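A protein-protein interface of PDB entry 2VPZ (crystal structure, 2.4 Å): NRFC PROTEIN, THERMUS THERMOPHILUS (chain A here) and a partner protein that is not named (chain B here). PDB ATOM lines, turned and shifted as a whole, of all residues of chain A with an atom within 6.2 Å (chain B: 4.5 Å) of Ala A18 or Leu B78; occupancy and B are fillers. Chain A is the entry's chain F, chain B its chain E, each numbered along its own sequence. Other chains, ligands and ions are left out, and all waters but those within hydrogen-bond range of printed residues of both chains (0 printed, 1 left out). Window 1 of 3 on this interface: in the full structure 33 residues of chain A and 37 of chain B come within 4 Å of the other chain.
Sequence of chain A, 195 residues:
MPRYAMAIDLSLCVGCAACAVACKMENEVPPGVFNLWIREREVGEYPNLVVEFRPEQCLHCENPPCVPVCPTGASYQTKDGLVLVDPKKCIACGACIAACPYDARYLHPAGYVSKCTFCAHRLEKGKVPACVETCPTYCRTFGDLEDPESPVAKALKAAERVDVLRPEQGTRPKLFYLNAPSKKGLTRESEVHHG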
ATOM      1  N   GLY A  15      22.241 -14.957 -12.121  1.00  0.00           N
ATOM      2  CA  GLY A  15      22.191 -14.774 -10.679  1.00  0.00           C
ATOM      3  C   GLY A  15      21.194 -13.775 -10.079  1.00  0.00           C
ATOM      4  O   GLY A  15      21.496 -13.133  -9.057  1.00  0.00           O
ATOM      5  N   CYS A  16      20.049 -13.612 -10.748  1.00  0.00           N
ATOM      6  CA  CYS A  16      18.873 -12.791 -10.346  1.00  0.00           C
ATOM      7  C   CYS A  16      18.448 -13.734  -9.194  1.00  0.00           C
ATOM      8  O   CYS A  16      18.674 -14.895  -9.361  1.00  0.00           O
ATOM      9  CB  CYS A  16      17.825 -12.908 -11.474  1.00  0.00           C
ATOM     10  SG  CYS A  16      17.328 -14.832 -11.735  1.00  0.00           S
ATOM     11  N   ALA A  17      17.870 -13.444  -8.055  1.00  0.00           N
ATOM     12  CA  ALA A  17      17.704 -14.720  -7.280  1.00  0.00           C
ATOM     13  C   ALA A  17      16.306 -15.360  -7.282  1.00  0.00           C
ATOM     14  O   ALA A  17      15.777 -15.707  -6.227  1.00  0.00           O
ATOM     15  CB  ALA A  17      18.214 -14.569  -5.830  1.00  0.00           C
ATOM     16  N   ALA A  18      15.744 -15.585  -8.466  1.00  0.00           N
ATOM     17  CA  ALA A  18      14.361 -16.077  -8.584  1.00  0.00           C
ATOM     18  C   ALA A  18      14.000 -17.448  -8.043  1.00  0.00           C
ATOM     19  O   ALA A  18      12.911 -17.636  -7.458  1.00  0.00           O
ATOM     20  CB  ALA A  18      13.871 -15.955 -10.016  1.00  0.00           C
ATOM     21  N   CYS A  19      14.909 -18.386  -8.284  1.00  0.00           N
ATOM     22  CA  CYS A  19      14.856 -19.777  -7.854  1.00  0.00           C
ATOM     23  C   CYS A  19      14.924 -19.730  -6.314  1.00  0.00           C
ATOM     24  O   CYS A  19      14.081 -20.309  -5.618  1.00  0.00           O
ATOM     25  CB  CYS A  19      16.044 -20.567  -8.455  1.00  0.00           C
ATOM     26  SG  CYS A  19      17.745 -19.914  -8.137  1.00  0.00           S
ATOM     27  N   ALA A  20      15.913 -19.010  -5.795  1.00  0.00           N
ATOM     28  CA  ALA A  20      16.080 -18.853  -4.359  1.00  0.00           C
ATOM     29  C   ALA A  20      14.804 -18.316  -3.676  1.00  0.00           C
ATOM     30  O   ALA A  20      14.412 -18.823  -2.623  1.00  0.00           O
ATOM     31  CB  ALA A  20      17.271 -17.932  -4.042  1.00  0.00           C
ATOM     32  N   VAL A  21      14.144 -17.312  -4.257  1.00  0.00           N
ATOM     33  CA  VAL A  21      12.920 -16.768  -3.661  1.00  0.00           C
ATOM     34  C   VAL A  21      11.711 -17.711  -3.872  1.00  0.00           C
ATOM     35  O   VAL A  21      10.896 -17.883  -2.964  1.00  0.00           O
ATOM     36  CB  VAL A  21      12.612 -15.265  -4.161  1.00  0.00           C
ATOM     37  CG1 VAL A  21      11.335 -14.695  -3.484  1.00  0.00           C
ATOM     38  CG2 VAL A  21      13.808 -14.340  -3.845  1.00  0.00           C
ATOM     39  N   ALA A  22      11.612 -18.356  -5.031  1.00  0.00           N
ATOM     40  CA  ALA A  22      10.526 -19.329  -5.300  1.00  0.00           C
ATOM     41  C   ALA A  22      10.538 -20.495  -4.240  1.00  0.00           C
ATOM     42  O   ALA A  22       9.470 -20.903  -3.732  1.00  0.00           O
ATOM     43  CB  ALA A  22      10.613 -19.865  -6.762  1.00  0.00           C
ATOM     44  N   CYS A  23      11.743 -20.994  -3.913  1.00  0.00           N
ATOM     45  CA  CYS A  23      12.005 -22.014  -2.861  1.00  0.00           C
ATOM     46  C   CYS A  23      11.433 -21.546  -1.482  1.00  0.00           C
ATOM     47  O   CYS A  23      10.607 -22.229  -0.896  1.00  0.00           O
ATOM     48  CB  CYS A  23      13.527 -22.273  -2.696  1.00  0.00           C
ATOM     49  SG  CYS A  23      13.952 -23.737  -1.595  1.00  0.00           S
ATOM     50  N   ALA A 130       9.951 -26.243  -7.814  1.00  0.00           N
ATOM     51  CA  ALA A 130       9.574 -24.822  -7.861  1.00  0.00           C
ATOM     52  C   ALA A 130      10.655 -23.868  -8.437  1.00  0.00           C
ATOM     53  O   ALA A 130      10.330 -22.877  -9.105  1.00  0.00           O
ATOM     54  CB  ALA A 130       9.163 -24.357  -6.469  1.00  0.00           C
ATOM     55  N   CYS A 131      11.923 -24.165  -8.166  1.00  0.00           N
ATOM     56  CA  CYS A 131      13.059 -23.378  -8.667  1.00  0.00           C
ATOM     57  C   CYS A 131      13.255 -23.561 -10.193  1.00  0.00           C
ATOM     58  O   CYS A 131      13.654 -22.632 -10.913  1.00  0.00           O
ATOM     59  CB  CYS A 131      14.349 -23.780  -7.935  1.00  0.00           C
ATOM     60  SG  CYS A 131      14.702 -25.580  -7.921  1.00  0.00           S
ATOM     61  N   GLU A 133      10.786 -24.482 -12.182  1.00  0.00           N
ATOM     62  CA  GLU A 133       9.573 -23.899 -12.769  1.00  0.00           C
ATOM     63  C   GLU A 133       9.651 -22.377 -13.040  1.00  0.00           C
ATOM     64  O   GLU A 133       9.312 -21.903 -14.126  1.00  0.00           O
ATOM     65  CB  GLU A 133       8.372 -24.161 -11.861  1.00  0.00           C
ATOM     66  CG  GLU A 133       7.123 -24.727 -12.518  1.00  0.00           C
ATOM     67  CD  GLU A 133       5.847 -24.308 -11.773  1.00  0.00           C
ATOM     68  OE1 GLU A 133       5.843 -24.360 -10.517  1.00  0.00           O
ATOM     69  OE2 GLU A 133       4.868 -23.925 -12.447  1.00  0.00           O
ATOM     70  N   THR A 134      10.095 -21.618 -12.048  1.00  0.00           N
ATOM     71  CA  THR A 134      10.196 -20.155 -12.144  1.00  0.00           C
ATOM     72  C   THR A 134      11.319 -19.565 -13.016  1.00  0.00           C
ATOM     73  O   THR A 134      11.224 -18.407 -13.449  1.00  0.00           O
ATOM     74  CB  THR A 134      10.450 -19.498 -10.761  1.00  0.00           C
ATOM     75  OG1 THR A 134      10.186 -18.101 -10.837  1.00  0.00           O
ATOM     76  CG2 THR A 134      11.930 -19.676 -10.372  1.00  0.00           C
ATOM     77  N   CYS A 135      12.372 -20.351 -13.255  1.00  0.00           N
ATOM     78  CA  CYS A 135      13.573 -19.852 -13.953  1.00  0.00           C
ATOM     79  C   CYS A 135      13.359 -19.138 -15.287  1.00  0.00           C
ATOM     80  O   CYS A 135      13.017 -19.749 -16.305  1.00  0.00           O
ATOM     81  CB  CYS A 135      14.748 -20.914 -14.064  1.00  0.00           C
ATOM     82  SG  CYS A 135      16.697 -20.143 -14.153  1.00  0.00           S
ATOM     83  N   PRO A 136      13.569 -17.802 -15.284  1.00  0.00           N
ATOM     84  CA  PRO A 136      13.432 -16.910 -16.429  1.00  0.00           C
ATOM     85  C   PRO A 136      14.432 -17.221 -17.543  1.00  0.00           C
ATOM     86  O   PRO A 136      14.087 -17.169 -18.732  1.00  0.00           O
ATOM     87  CB  PRO A 136      13.663 -15.520 -15.823  1.00  0.00           C
ATOM     88  CG  PRO A 136      13.241 -15.691 -14.409  1.00  0.00           C
ATOM     89  CD  PRO A 136      13.917 -17.010 -14.100  1.00  0.00           C
ATOM     90  N   ILE B  53      -0.226 -13.480 -13.570  1.00  0.00           N
ATOM     91  CA  ILE B  53       0.111 -14.534 -12.613  1.00  0.00           C
ATOM     92  C   ILE B  53      -1.084 -15.353 -12.107  1.00  0.00           C
ATOM     93  O   ILE B  53      -2.227 -15.051 -12.440  1.00  0.00           O
ATOM     94  CB  ILE B  53       0.820 -13.868 -11.340  1.00  0.00           C
ATOM     95  CG1 ILE B  53      -0.124 -12.855 -10.678  1.00  0.00           C
ATOM     96  CG2 ILE B  53       2.138 -13.168 -11.747  1.00  0.00           C
ATOM     97  CD1 ILE B  53       0.281 -12.331  -9.269  1.00  0.00           C
ATOM     98  N   VAL B  65       2.736 -17.530  -5.643  1.00  0.00           N
ATOM     99  CA  VAL B  65       2.240 -16.872  -6.834  1.00  0.00           C
ATOM    100  C   VAL B  65       3.031 -17.520  -8.014  1.00  0.00           C
ATOM    101  O   VAL B  65       4.173 -17.942  -7.832  1.00  0.00           O
ATOM    102  CB  VAL B  65       2.388 -15.316  -6.640  1.00  0.00           C
ATOM    103  CG1 VAL B  65       3.471 -14.736  -7.552  1.00  0.00           C
ATOM    104  CG2 VAL B  65       0.994 -14.636  -6.764  1.00  0.00           C
ATOM    105  N   GLU B  66       2.434 -17.664  -9.192  1.00  0.00           N
ATOM    106  CA  GLU B  66       3.125 -18.334 -10.307  1.00  0.00           C
ATOM    107  C   GLU B  66       2.802 -17.727 -11.680  1.00  0.00           C
ATOM    108  O   GLU B  66       1.707 -17.202 -11.867  1.00  0.00           O
ATOM    109  CB  GLU B  66       2.751 -19.834 -10.328  1.00  0.00           C
ATOM    110  CG  GLU B  66       3.831 -20.800 -10.872  1.00  0.00           C
ATOM    111  CD  GLU B  66       4.976 -21.109  -9.861  1.00  0.00           C
ATOM    112  OE1 GLU B  66       4.689 -21.654  -8.771  1.00  0.00           O
ATOM    113  OE2 GLU B  66       6.153 -20.796 -10.167  1.00  0.00           O
ATOM    114  N   GLY B  67       3.740 -17.776 -12.618  1.00  0.00           N
ATOM    115  CA  GLY B  67       3.476 -17.277 -13.951  1.00  0.00           C
ATOM    116  C   GLY B  67       2.583 -18.305 -14.648  1.00  0.00           C
ATOM    117  O   GLY B  67       2.387 -19.379 -14.089  1.00  0.00           O
ATOM    118  N   SER B  74       4.487 -13.427 -18.619  1.00  0.00           N
ATOM    119  CA  SER B  74       5.181 -14.390 -17.765  1.00  0.00           C
ATOM    120  C   SER B  74       5.493 -15.814 -18.368  1.00  0.00           C
ATOM    121  O   SER B  74       6.492 -16.439 -17.966  1.00  0.00           O
ATOM    122  CB  SER B  74       4.481 -14.537 -16.385  1.00  0.00           C
ATOM    123  OG  SER B  74       3.221 -15.138 -16.456  1.00  0.00           O
ATOM    124  N   ARG B  77       7.008 -18.532 -16.203  1.00  0.00           N
ATOM    125  CA  ARG B  77       8.127 -18.087 -15.368  1.00  0.00           C
ATOM    126  C   ARG B  77       7.857 -16.778 -14.560  1.00  0.00           C
ATOM    127  O   ARG B  77       6.871 -16.078 -14.820  1.00  0.00           O
ATOM    128  CB  ARG B  77       9.373 -17.942 -16.274  1.00  0.00           C
ATOM    129  CG  ARG B  77       9.537 -19.058 -17.360  1.00  0.00           C
ATOM    130  CD  ARG B  77       9.822 -20.411 -16.678  1.00  0.00           C
ATOM    131  NE  ARG B  77      10.087 -21.563 -17.551  1.00  0.00           N
ATOM    132  CZ  ARG B  77      11.161 -22.363 -17.519  1.00  0.00           C
ATOM    133  NH1 ARG B  77      12.154 -22.163 -16.656  1.00  0.00           N
ATOM    134  NH2 ARG B  77      11.229 -23.414 -18.336  1.00  0.00           N
ATOM    135  N   LEU B  78       8.708 -16.457 -13.584  1.00  0.00           N
ATOM    136  CA  LEU B  78       8.537 -15.248 -12.781  1.00  0.00           C
ATOM    137  C   LEU B  78       9.886 -14.738 -12.282  1.00  0.00           C
ATOM    138  O   LEU B  78      10.818 -15.519 -12.166  1.00  0.00           O
ATOM    139  CB  LEU B  78       7.624 -15.534 -11.591  1.00  0.00           C
ATOM    140  CG  LEU B  78       6.511 -14.518 -11.328  1.00  0.00           C
ATOM    141  CD1 LEU B  78       5.489 -14.401 -12.500  1.00  0.00           C
ATOM    142  CD2 LEU B  78       5.824 -14.976 -10.055  1.00  0.00           C
ATOM    143  N   CYS B  79      10.022 -13.450 -11.988  1.00  0.00           N
ATOM    144  CA  CYS B  79      11.311 -12.994 -11.481  1.00  0.00           C
ATOM    145  C   CYS B  79      11.323 -13.081  -9.925  1.00  0.00           C
ATOM    146  O   CYS B  79      10.292 -13.433  -9.327  1.00  0.00           O
ATOM    147  CB  CYS B  79      11.644 -11.566 -11.989  1.00  0.00           C
ATOM    148  SG  CYS B  79      10.912 -10.134 -11.058  1.00  0.00           S
ATOM    149  N   PRO B  80      12.478 -12.787  -9.259  1.00  0.00           N
ATOM    150  CA  PRO B  80      12.542 -12.855  -7.786  1.00  0.00           C
ATOM    151  C   PRO B  80      11.532 -11.964  -7.003  1.00  0.00           C
ATOM    152  O   PRO B  80      10.920 -12.399  -6.015  1.00  0.00           O
ATOM    153  CB  PRO B  80      14.007 -12.522  -7.444  1.00  0.00           C
ATOM    154  CG  PRO B  80      14.616 -11.979  -8.689  1.00  0.00           C
ATOM    155  CD  PRO B  80      13.728 -12.303  -9.858  1.00  0.00           C
ATOM    156  N   GLY B  82       8.622 -10.752  -8.124  1.00  0.00           N
ATOM    157  CA  GLY B  82       7.262 -11.231  -8.283  1.00  0.00           C
ATOM    158  C   GLY B  82       6.952 -12.335  -7.273  1.00  0.00           C
ATOM    159  O   GLY B  82       5.851 -12.391  -6.713  1.00  0.00           O
ATOM    160  N   GLN B  83       7.929 -13.207  -7.018  1.00  0.00           N
ATOM    161  CA  GLN B  83       7.757 -14.321  -6.071  1.00  0.00           C
ATOM    162  C   GLN B  83       7.644 -13.838  -4.615  1.00  0.00           C
ATOM    163  O   GLN B  83       6.912 -14.423  -3.824  1.00  0.00           O
ATOM    164  CB  GLN B  83       8.914 -15.349  -6.181  1.00  0.00           C
ATOM    165  CG  GLN B  83       9.033 -16.122  -7.512  1.00  0.00           C
ATOM    166  CD  GLN B  83       8.124 -17.357  -7.608  1.00  0.00           C
ATOM    167  OE1 GLN B  83       7.929 -17.926  -8.691  1.00  0.00           O
ATOM    168  NE2 GLN B  83       7.574 -17.778  -6.467  1.00  0.00           N
ATOM    169  N   ASN B 216      10.854  -9.435 -16.322  1.00  0.00           N
ATOM    170  CA  ASN B 216      10.644 -10.835 -16.678  1.00  0.00           C
ATOM    171  C   ASN B 216      10.751 -11.321 -18.153  1.00  0.00           C
ATOM    172  O   ASN B 216      11.657 -12.096 -18.486  1.00  0.00           O
ATOM    173  CB  ASN B 216       9.356 -11.289 -15.943  1.00  0.00           C
ATOM    174  CG  ASN B 216       9.092 -12.788 -15.985  1.00  0.00           C
ATOM    175  OD1 ASN B 216       9.992 -13.599 -16.209  1.00  0.00           O
ATOM    176  ND2 ASN B 216       7.830 -13.164 -15.751  1.00  0.00           N
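NH1 of Arg B77 sits at hydrogen-bond distance from O of Cys A135, at 2.6 Å. OG1 of Thr A134 is in hydrogen-bond range of OE1 of Gln B83 (3.1 Å). The side-chain carboxylate (OE1) of Glu A133 lies close to the side-chain carboxylate (OE1) of Glu B66, at 3.4 Å. OG1 of Thr A134 sits at hydrogen-bond distance from O of Leu B78 (3.0 Å).
SG of Cys B79 lies close to N of Gly B82 (3.8 Å). ND2 of Asn B216 sits at hydrogen-bond distance from O of Arg B77, at 3.2 Å. N of Ala A18 sits close to SG of Cys A16, 3.7 Å away.
Among the printed residues, pairs that only touch across the chains: Glu A133 with Arg B77 (3.0 Å), Pro A136 with Leu B78 (3.3 Å), Thr A134 with Arg B77 (3.4 Å), Val A21 with Pro B80 (3.4 Å), Ala A22 with Gln B83 (3.5 Å), Ala A18 with Pro B80 (3.5 Å), Ala A17 with Pro B80 (3.6 Å), Val A21 with Gln B83 (3.7 Å), Ala A18 with Leu B78 (3.8 Å) and Ala A18 with Cys B79 (3.8 Å).
Gly A15 touches none of the printed residues of chain B. Printed residues of chain B within 4 Å of Ala A17: Pro B80. Ala A18 touches three residues of chain B. Printed residues of chain B within 4 Å of Ala A22: Gln B83 (3.5 Å). Of the printed residues of chain B, Thr A134 touches Arg B77 (3.4 Å), Leu B78 (3.0 Å) and Gln B83 (3.1 Å). Of the printed residues of chain B, Pro A136 touches Leu B78 (3.3 Å). Leu B78 touches three residues of chain A. Asn B216 touches none of the printed residues of chain A. The nearest printed residue of chain A that does not touch Arg B77 is Pro A136 (4.2 Å).
Of the 15 printed residues of chain A, 8 touch a printed residue of chain B. Printed residues of chain A that touch a printed residue of chain B: Ala A17, Ala A18, Val A21, Ala A22, Glu A133, Thr A134, Cys A135 and Pro A136. Hydrophobic or aromatic side chains of chain A within 4 Å of the printed part of chain B: Ala A18, Val A21, Ala A22 and Pro A136. Printed residues of chain B that touch a printed residue of chain A: Glu B66, Arg B77, Leu B78, Cys B79, Pro B80 and Gln B83.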
